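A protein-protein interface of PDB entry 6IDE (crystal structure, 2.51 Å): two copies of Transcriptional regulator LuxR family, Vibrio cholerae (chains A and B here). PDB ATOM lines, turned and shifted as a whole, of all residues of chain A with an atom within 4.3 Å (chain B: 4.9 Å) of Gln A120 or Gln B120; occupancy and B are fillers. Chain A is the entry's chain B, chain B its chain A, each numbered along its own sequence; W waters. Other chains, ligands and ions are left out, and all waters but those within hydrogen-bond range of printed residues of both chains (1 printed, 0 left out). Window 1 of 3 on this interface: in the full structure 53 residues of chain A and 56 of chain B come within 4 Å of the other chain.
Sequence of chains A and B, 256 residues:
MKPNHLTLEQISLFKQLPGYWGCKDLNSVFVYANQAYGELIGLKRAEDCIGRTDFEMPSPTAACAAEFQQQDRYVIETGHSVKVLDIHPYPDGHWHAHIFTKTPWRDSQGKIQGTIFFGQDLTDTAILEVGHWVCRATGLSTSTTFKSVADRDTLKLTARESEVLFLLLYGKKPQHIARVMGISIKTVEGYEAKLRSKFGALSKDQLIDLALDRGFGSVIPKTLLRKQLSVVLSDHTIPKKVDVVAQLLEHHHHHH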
ATOM      1  N   LYS A  83       4.090   1.706  -1.887  1.00  0.00           N
ATOM      2  CA  LYS A  83       4.876   0.496  -2.073  1.00  0.00           C
ATOM      3  C   LYS A  83       3.927  -0.691  -2.060  1.00  0.00           C
ATOM      4  O   LYS A  83       3.112  -0.833  -1.143  1.00  0.00           O
ATOM      5  CB  LYS A  83       5.953   0.368  -0.984  1.00  0.00           C
ATOM      6  CG  LYS A  83       6.891   1.564  -0.962  1.00  0.00           C
ATOM      7  CD  LYS A  83       7.992   1.455   0.077  1.00  0.00           C
ATOM      8  CE  LYS A  83       9.031   0.445  -0.294  1.00  0.00           C
ATOM      9  NZ  LYS A  83      10.250   0.614   0.560  1.00  0.00           N
ATOM     10  N   HIS A  98       7.692  -9.432  -5.682  1.00  0.00           N
ATOM     11  CA  HIS A  98       8.336  -8.155  -5.928  1.00  0.00           C
ATOM     12  C   HIS A  98       7.802  -7.131  -4.947  1.00  0.00           C
ATOM     13  O   HIS A  98       6.752  -7.330  -4.327  1.00  0.00           O
ATOM     14  CB  HIS A  98       8.084  -7.637  -7.352  1.00  0.00           C
ATOM     15  CG  HIS A  98       8.695  -8.477  -8.428  1.00  0.00           C
ATOM     16  ND1 HIS A  98       8.037  -9.541  -9.004  1.00  0.00           N
ATOM     17  CD2 HIS A  98       9.892  -8.392  -9.053  1.00  0.00           C
ATOM     18  CE1 HIS A  98       8.808 -10.088  -9.928  1.00  0.00           C
ATOM     19  NE2 HIS A  98       9.942  -9.412  -9.975  1.00  0.00           N
ATOM     20  N   ILE A  99       8.526  -6.018  -4.842  1.00  0.00           N
ATOM     21  CA  ILE A  99       8.035  -4.797  -4.213  1.00  0.00           C
ATOM     22  C   ILE A  99       8.031  -3.707  -5.280  1.00  0.00           C
ATOM     23  O   ILE A  99       9.094  -3.279  -5.748  1.00  0.00           O
ATOM     24  CB  ILE A  99       8.879  -4.379  -3.005  1.00  0.00           C
ATOM     25  CG1 ILE A  99       8.933  -5.512  -1.963  1.00  0.00           C
ATOM     26  CG2 ILE A  99       8.310  -3.118  -2.393  1.00  0.00           C
ATOM     27  CD1 ILE A  99       7.633  -5.787  -1.294  1.00  0.00           C
ATOM     28  N   THR A 101       7.367   0.057  -6.265  1.00  0.00           N
ATOM     29  CA  THR A 101       7.185   1.436  -5.839  1.00  0.00           C
ATOM     30  C   THR A 101       6.466   2.173  -6.951  1.00  0.00           C
ATOM     31  O   THR A 101       6.812   2.010  -8.123  1.00  0.00           O
ATOM     32  CB  THR A 101       8.526   2.118  -5.552  1.00  0.00           C
ATOM     33  OG1 THR A 101       9.253   1.342  -4.603  1.00  0.00           O
ATOM     34  CG2 THR A 101       8.318   3.540  -5.006  1.00  0.00           C
ATOM     35  N   PHE A 118       8.424   1.044 -10.161  1.00  0.00           N
ATOM     36  CA  PHE A 118       9.768   0.485 -10.033  1.00  0.00           C
ATOM     37  C   PHE A 118       9.685  -0.766  -9.171  1.00  0.00           C
ATOM     38  O   PHE A 118       9.481  -0.675  -7.954  1.00  0.00           O
ATOM     39  CB  PHE A 118      10.752   1.501  -9.442  1.00  0.00           C
ATOM     40  CG  PHE A 118      12.169   0.999  -9.382  1.00  0.00           C
ATOM     41  CD1 PHE A 118      12.626   0.309  -8.269  1.00  0.00           C
ATOM     42  CD2 PHE A 118      13.034   1.202 -10.441  1.00  0.00           C
ATOM     43  CE1 PHE A 118      13.917  -0.169  -8.216  1.00  0.00           C
ATOM     44  CE2 PHE A 118      14.326   0.731 -10.398  1.00  0.00           C
ATOM     45  CZ  PHE A 118      14.767   0.035  -9.286  1.00  0.00           C
ATOM     46  N   GLY A 119       9.848  -1.925  -9.801  1.00  0.00           N
ATOM     47  CA  GLY A 119       9.830  -3.205  -9.109  1.00  0.00           C
ATOM     48  C   GLY A 119      11.211  -3.714  -8.780  1.00  0.00           C
ATOM     49  O   GLY A 119      12.129  -3.665  -9.604  1.00  0.00           O
ATOM     50  N   GLN A 120      11.365  -4.220  -7.559  1.00  0.00           N
ATOM     51  CA  GLN A 120      12.555  -4.924  -7.119  1.00  0.00           C
ATOM     52  C   GLN A 120      12.196  -6.337  -6.685  1.00  0.00           C
ATOM     53  O   GLN A 120      11.208  -6.541  -5.968  1.00  0.00           O
ATOM     54  CB  GLN A 120      13.223  -4.203  -5.956  1.00  0.00           C
ATOM     55  CG  GLN A 120      14.314  -3.265  -6.387  1.00  0.00           C
ATOM     56  CD  GLN A 120      15.142  -2.793  -5.222  1.00  0.00           C
ATOM     57  OE1 GLN A 120      14.614  -2.591  -4.124  1.00  0.00           O
ATOM     58  NE2 GLN A 120      16.450  -2.617  -5.445  1.00  0.00           N
ATOM     59  N   ASP A 121      13.007  -7.308  -7.112  1.00  0.00           N
ATOM     60  CA  ASP A 121      12.876  -8.661  -6.586  1.00  0.00           C
ATOM     61  C   ASP A 121      12.950  -8.624  -5.067  1.00  0.00           C
ATOM     62  O   ASP A 121      13.645  -7.786  -4.487  1.00  0.00           O
ATOM     63  CB  ASP A 121      13.975  -9.568  -7.146  1.00  0.00           C
ATOM     64  CG  ASP A 121      13.851  -9.794  -8.649  1.00  0.00           C
ATOM     65  OD1 ASP A 121      12.840 -10.381  -9.087  1.00  0.00           O
ATOM     66  OD2 ASP A 121      14.771  -9.395  -9.394  1.00  0.00           O
ATOM     67  N   LEU A 122      12.203  -9.518  -4.417  1.00  0.00           N
ATOM     68  CA  LEU A 122      12.148  -9.480  -2.960  1.00  0.00           C
ATOM     69  C   LEU A 122      13.521  -9.715  -2.356  1.00  0.00           C
ATOM     70  O   LEU A 122      13.838  -9.145  -1.306  1.00  0.00           O
ATOM     71  CB  LEU A 122      11.149 -10.513  -2.434  1.00  0.00           C
ATOM     72  CG  LEU A 122      10.336 -10.242  -1.159  1.00  0.00           C
ATOM     73  CD1 LEU A 122      10.938 -10.925   0.028  1.00  0.00           C
ATOM     74  CD2 LEU A 122      10.186  -8.754  -0.885  1.00  0.00           C
ATOM     75  N   ASP A 124      16.359  -8.629  -3.315  1.00  0.00           N
ATOM     76  CA  ASP A 124      17.106  -7.381  -3.280  1.00  0.00           C
ATOM     77  C   ASP A 124      16.514  -6.367  -2.305  1.00  0.00           C
ATOM     78  O   ASP A 124      16.849  -5.178  -2.381  1.00  0.00           O
ATOM     79  CB  ASP A 124      17.182  -6.773  -4.683  1.00  0.00           C
ATOM     80  CG  ASP A 124      17.851  -7.697  -5.686  1.00  0.00           C
ATOM     81  OD1 ASP A 124      18.890  -8.305  -5.339  1.00  0.00           O
ATOM     82  OD2 ASP A 124      17.336  -7.831  -6.821  1.00  0.00           O
ATOM     83  N   THR A 125      15.630  -6.802  -1.410  1.00  0.00           N
ATOM     84  CA  THR A 125      15.041  -5.939  -0.396  1.00  0.00           C
ATOM     85  C   THR A 125      15.325  -6.520   0.984  1.00  0.00           C
ATOM     86  O   THR A 125      15.724  -7.680   1.135  1.00  0.00           O
ATOM     87  CB  THR A 125      13.515  -5.752  -0.604  1.00  0.00           C
ATOM     88  OG1 THR A 125      12.789  -6.928  -0.207  1.00  0.00           O
ATOM     89  CG2 THR A 125      13.197  -5.433  -2.059  1.00  0.00           C
ATOM     90  N   TYR B  20      17.638   6.743  -4.931  1.00  0.00           N
ATOM     91  CA  TYR B  20      18.893   7.495  -4.853  1.00  0.00           C
ATOM     92  C   TYR B  20      19.943   6.651  -5.567  1.00  0.00           C
ATOM     93  O   TYR B  20      20.387   5.627  -5.041  1.00  0.00           O
ATOM     94  CB  TYR B  20      19.276   7.770  -3.403  1.00  0.00           C
ATOM     95  CG  TYR B  20      18.156   8.394  -2.597  1.00  0.00           C
ATOM     96  CD1 TYR B  20      17.137   7.610  -2.067  1.00  0.00           C
ATOM     97  CD2 TYR B  20      18.113   9.772  -2.379  1.00  0.00           C
ATOM     98  CE1 TYR B  20      16.105   8.176  -1.339  1.00  0.00           C
ATOM     99  CE2 TYR B  20      17.089  10.350  -1.647  1.00  0.00           C
ATOM    100  CZ  TYR B  20      16.085   9.538  -1.126  1.00  0.00           C
ATOM    101  OH  TYR B  20      15.056  10.092  -0.397  1.00  0.00           O
ATOM    102  N   ALA B  97      17.826   5.381   7.195  1.00  0.00           N
ATOM    103  CA  ALA B  97      18.165   3.993   6.927  1.00  0.00           C
ATOM    104  C   ALA B  97      17.853   3.705   5.465  1.00  0.00           C
ATOM    105  O   ALA B  97      16.700   3.815   5.039  1.00  0.00           O
ATOM    106  CB  ALA B  97      17.392   3.053   7.856  1.00  0.00           C
ATOM    107  N   HIS B  98      18.879   3.356   4.696  1.00  0.00           N
ATOM    108  CA  HIS B  98      18.703   3.001   3.299  1.00  0.00           C
ATOM    109  C   HIS B  98      19.173   1.577   3.056  1.00  0.00           C
ATOM    110  O   HIS B  98      20.008   1.044   3.788  1.00  0.00           O
ATOM    111  CB  HIS B  98      19.481   3.938   2.368  1.00  0.00           C
ATOM    112  CG  HIS B  98      19.074   5.370   2.472  1.00  0.00           C
ATOM    113  ND1 HIS B  98      18.404   6.028   1.465  1.00  0.00           N
ATOM    114  CD2 HIS B  98      19.238   6.269   3.469  1.00  0.00           C
ATOM    115  CE1 HIS B  98      18.177   7.275   1.836  1.00  0.00           C
ATOM    116  NE2 HIS B  98      18.678   7.449   3.045  1.00  0.00           N
ATOM    117  N   ILE B  99      18.616   0.967   2.023  1.00  0.00           N
ATOM    118  CA  ILE B  99      19.174  -0.229   1.411  1.00  0.00           C
ATOM    119  C   ILE B  99      19.731   0.193   0.059  1.00  0.00           C
ATOM    120  O   ILE B  99      18.980   0.605  -0.838  1.00  0.00           O
ATOM    121  CB  ILE B  99      18.131  -1.338   1.250  1.00  0.00           C
ATOM    122  CG1 ILE B  99      17.695  -1.869   2.615  1.00  0.00           C
ATOM    123  CG2 ILE B  99      18.702  -2.435   0.373  1.00  0.00           C
ATOM    124  CD1 ILE B  99      18.792  -2.580   3.387  1.00  0.00           C
ATOM    125  N   THR B 101      21.522  -1.062  -3.282  1.00  0.00           N
ATOM    126  CA  THR B 101      21.808  -2.193  -4.141  1.00  0.00           C
ATOM    127  C   THR B 101      22.911  -1.758  -5.092  1.00  0.00           C
ATOM    128  O   THR B 101      22.856  -0.656  -5.647  1.00  0.00           O
ATOM    129  CB  THR B 101      20.532  -2.609  -4.889  1.00  0.00           C
ATOM    130  OG1 THR B 101      19.689  -3.340  -3.989  1.00  0.00           O
ATOM    131  CG2 THR B 101      20.825  -3.463  -6.121  1.00  0.00           C
ATOM    132  N   PHE B 118      21.993   1.875  -6.180  1.00  0.00           N
ATOM    133  CA  PHE B 118      20.577   2.218  -6.189  1.00  0.00           C
ATOM    134  C   PHE B 118      20.074   2.071  -4.762  1.00  0.00           C
ATOM    135  O   PHE B 118      20.023   0.959  -4.229  1.00  0.00           O
ATOM    136  CB  PHE B 118      19.781   1.332  -7.156  1.00  0.00           C
ATOM    137  CG  PHE B 118      18.354   1.767  -7.328  1.00  0.00           C
ATOM    138  CD1 PHE B 118      18.000   2.626  -8.356  1.00  0.00           C
ATOM    139  CD2 PHE B 118      17.376   1.338  -6.445  1.00  0.00           C
ATOM    140  CE1 PHE B 118      16.688   3.044  -8.504  1.00  0.00           C
ATOM    141  CE2 PHE B 118      16.077   1.756  -6.579  1.00  0.00           C
ATOM    142  CZ  PHE B 118      15.737   2.623  -7.606  1.00  0.00           C
ATOM    143  N   GLY B 119      19.713   3.190  -4.147  1.00  0.00           N
ATOM    144  CA  GLY B 119      19.317   3.229  -2.752  1.00  0.00           C
ATOM    145  C   GLY B 119      17.845   3.556  -2.588  1.00  0.00           C
ATOM    146  O   GLY B 119      17.284   4.354  -3.337  1.00  0.00           O
ATOM    147  N   GLN B 120      17.231   2.945  -1.587  1.00  0.00           N
ATOM    148  CA  GLN B 120      15.853   3.221  -1.246  1.00  0.00           C
ATOM    149  C   GLN B 120      15.771   3.521   0.237  1.00  0.00           C
ATOM    150  O   GLN B 120      16.344   2.794   1.054  1.00  0.00           O
ATOM    151  CB  GLN B 120      14.942   2.046  -1.618  1.00  0.00           C
ATOM    152  CG  GLN B 120      14.746   1.881  -3.119  1.00  0.00           C
ATOM    153  CD  GLN B 120      13.458   1.180  -3.456  1.00  0.00           C
ATOM    154  OE1 GLN B 120      12.825   1.474  -4.467  1.00  0.00           O
ATOM    155  NE2 GLN B 120      13.056   0.245  -2.606  1.00  0.00           N
ATOM    156  N   ASP B 121      15.082   4.606   0.575  1.00  0.00           N
ATOM    157  CA  ASP B 121      14.906   4.982   1.965  1.00  0.00           C
ATOM    158  C   ASP B 121      13.805   4.130   2.569  1.00  0.00           C
ATOM    159  O   ASP B 121      12.712   4.037   2.005  1.00  0.00           O
ATOM    160  CB  ASP B 121      14.554   6.465   2.079  1.00  0.00           C
ATOM    161  CG  ASP B 121      14.729   6.994   3.487  1.00  0.00           C
ATOM    162  OD1 ASP B 121      14.233   6.343   4.430  1.00  0.00           O
ATOM    163  OD2 ASP B 121      15.376   8.050   3.652  1.00  0.00           O
ATOM    164  N   LEU B 122      14.090   3.492   3.707  1.00  0.00           N
ATOM    165  CA  LEU B 122      13.032   2.778   4.407  1.00  0.00           C
ATOM    166  C   LEU B 122      12.857   3.250   5.842  1.00  0.00           C
ATOM    167  O   LEU B 122      12.230   2.545   6.636  1.00  0.00           O
ATOM    168  CB  LEU B 122      13.251   1.264   4.363  1.00  0.00           C
ATOM    169  CG  LEU B 122      14.622   0.634   4.530  1.00  0.00           C
ATOM    170  CD1 LEU B 122      15.191   0.904   5.899  1.00  0.00           C
ATOM    171  CD2 LEU B 122      14.502  -0.864   4.281  1.00  0.00           C
HETATM  172  O   HOH W   1      17.891  -1.268  -3.097  1.00  0.00           O
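Water W1 lies within hydrogen-bond range of OG1 of Thr B101 (2.9 Å), NE2 of Gln A120 (3.1 Å), O of Ile B99 (3.1 Å) and O of Phe B118 (3.3 Å).
Of the 10 printed residues of chain B, 3 touch a printed residue of chain A. Along chain B the printed residues that touch a printed residue of chain A span positions 101 to 120. Hydrophobic or aromatic side chains of chain A that line the printed part of chain B: Phe A118. Among the printed residues, 6 pairs touch across the chains. Among the printed residues, no Asp or Glu carboxylate lies within 4 Å of a Lys or Arg side-chain nitrogen of the other chain.
Thr A101 touches Gln B120, and with the chains exchanged Gln A120 touches Thr B101. Phe A118 touches its own counterpart, Phe B118. Phe A118 touches Gln B120, but with the chains exchanged Gln A120 does not touch Phe B118 (4.2 Å). Gln B120 touches its own counterpart, Gln A120. Positions printed for both chains: 98, 99, 101, 118, 119, 120, 121 and 122. Of the 6 pairs that touch across the chains among the printed residues, 4 have their exchanged pair printed and touching as well.
The backbone carbonyl oxygen of Phe B118 lies within hydrogen-bond range of the backbone NH of Thr B101. The backbone carbonyl oxygen of Ile B99 is in hydrogen-bond range of the backbone NH of Gln B120, at 3.0 Å. The backbone NH of Ile A99 lies within hydrogen-bond range of the backbone carbonyl oxygen of Gln A120, at 3.0 Å. The backbone NH of Phe A118 lies within hydrogen-bond range of the backbone carbonyl oxygen of Thr A101.
Printed residues of chain B within 4 Å of Phe A118: Phe B118 and Gln B120. Printed residues of chain B within 4 Å of Asp A124: Thr B101 (3.7 Å). Of the printed residues of chain A, Thr B101 touches Gln A120 and Asp A124. Of the printed residues of chain A, Gln B120 touches Thr A101 (3.6 Å), Phe A118 (3.98 Å) and Gln A120 (3.6 Å). The nearest residue of chain B that does not touch Gln A120 is Phe B118 (4.2 Å). The nearest printed residue of chain A that does not touch Gln B120 is Lys A83 (4.2 Å).
Gln B120 touches Thr A101. CZ of Phe B118 touches CZ of Phe A118, 3.2 Å away. Phe A118 touches Gln B120 (CD1 to OE1, 3.98 Å). NE2 of Gln A120 touches OG1 of Thr B101, at 3.6 Å. Gln B120 touches Gln A120 (NE2 to OE1, 3.6 Å). Thr B101 touches Asp A124.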
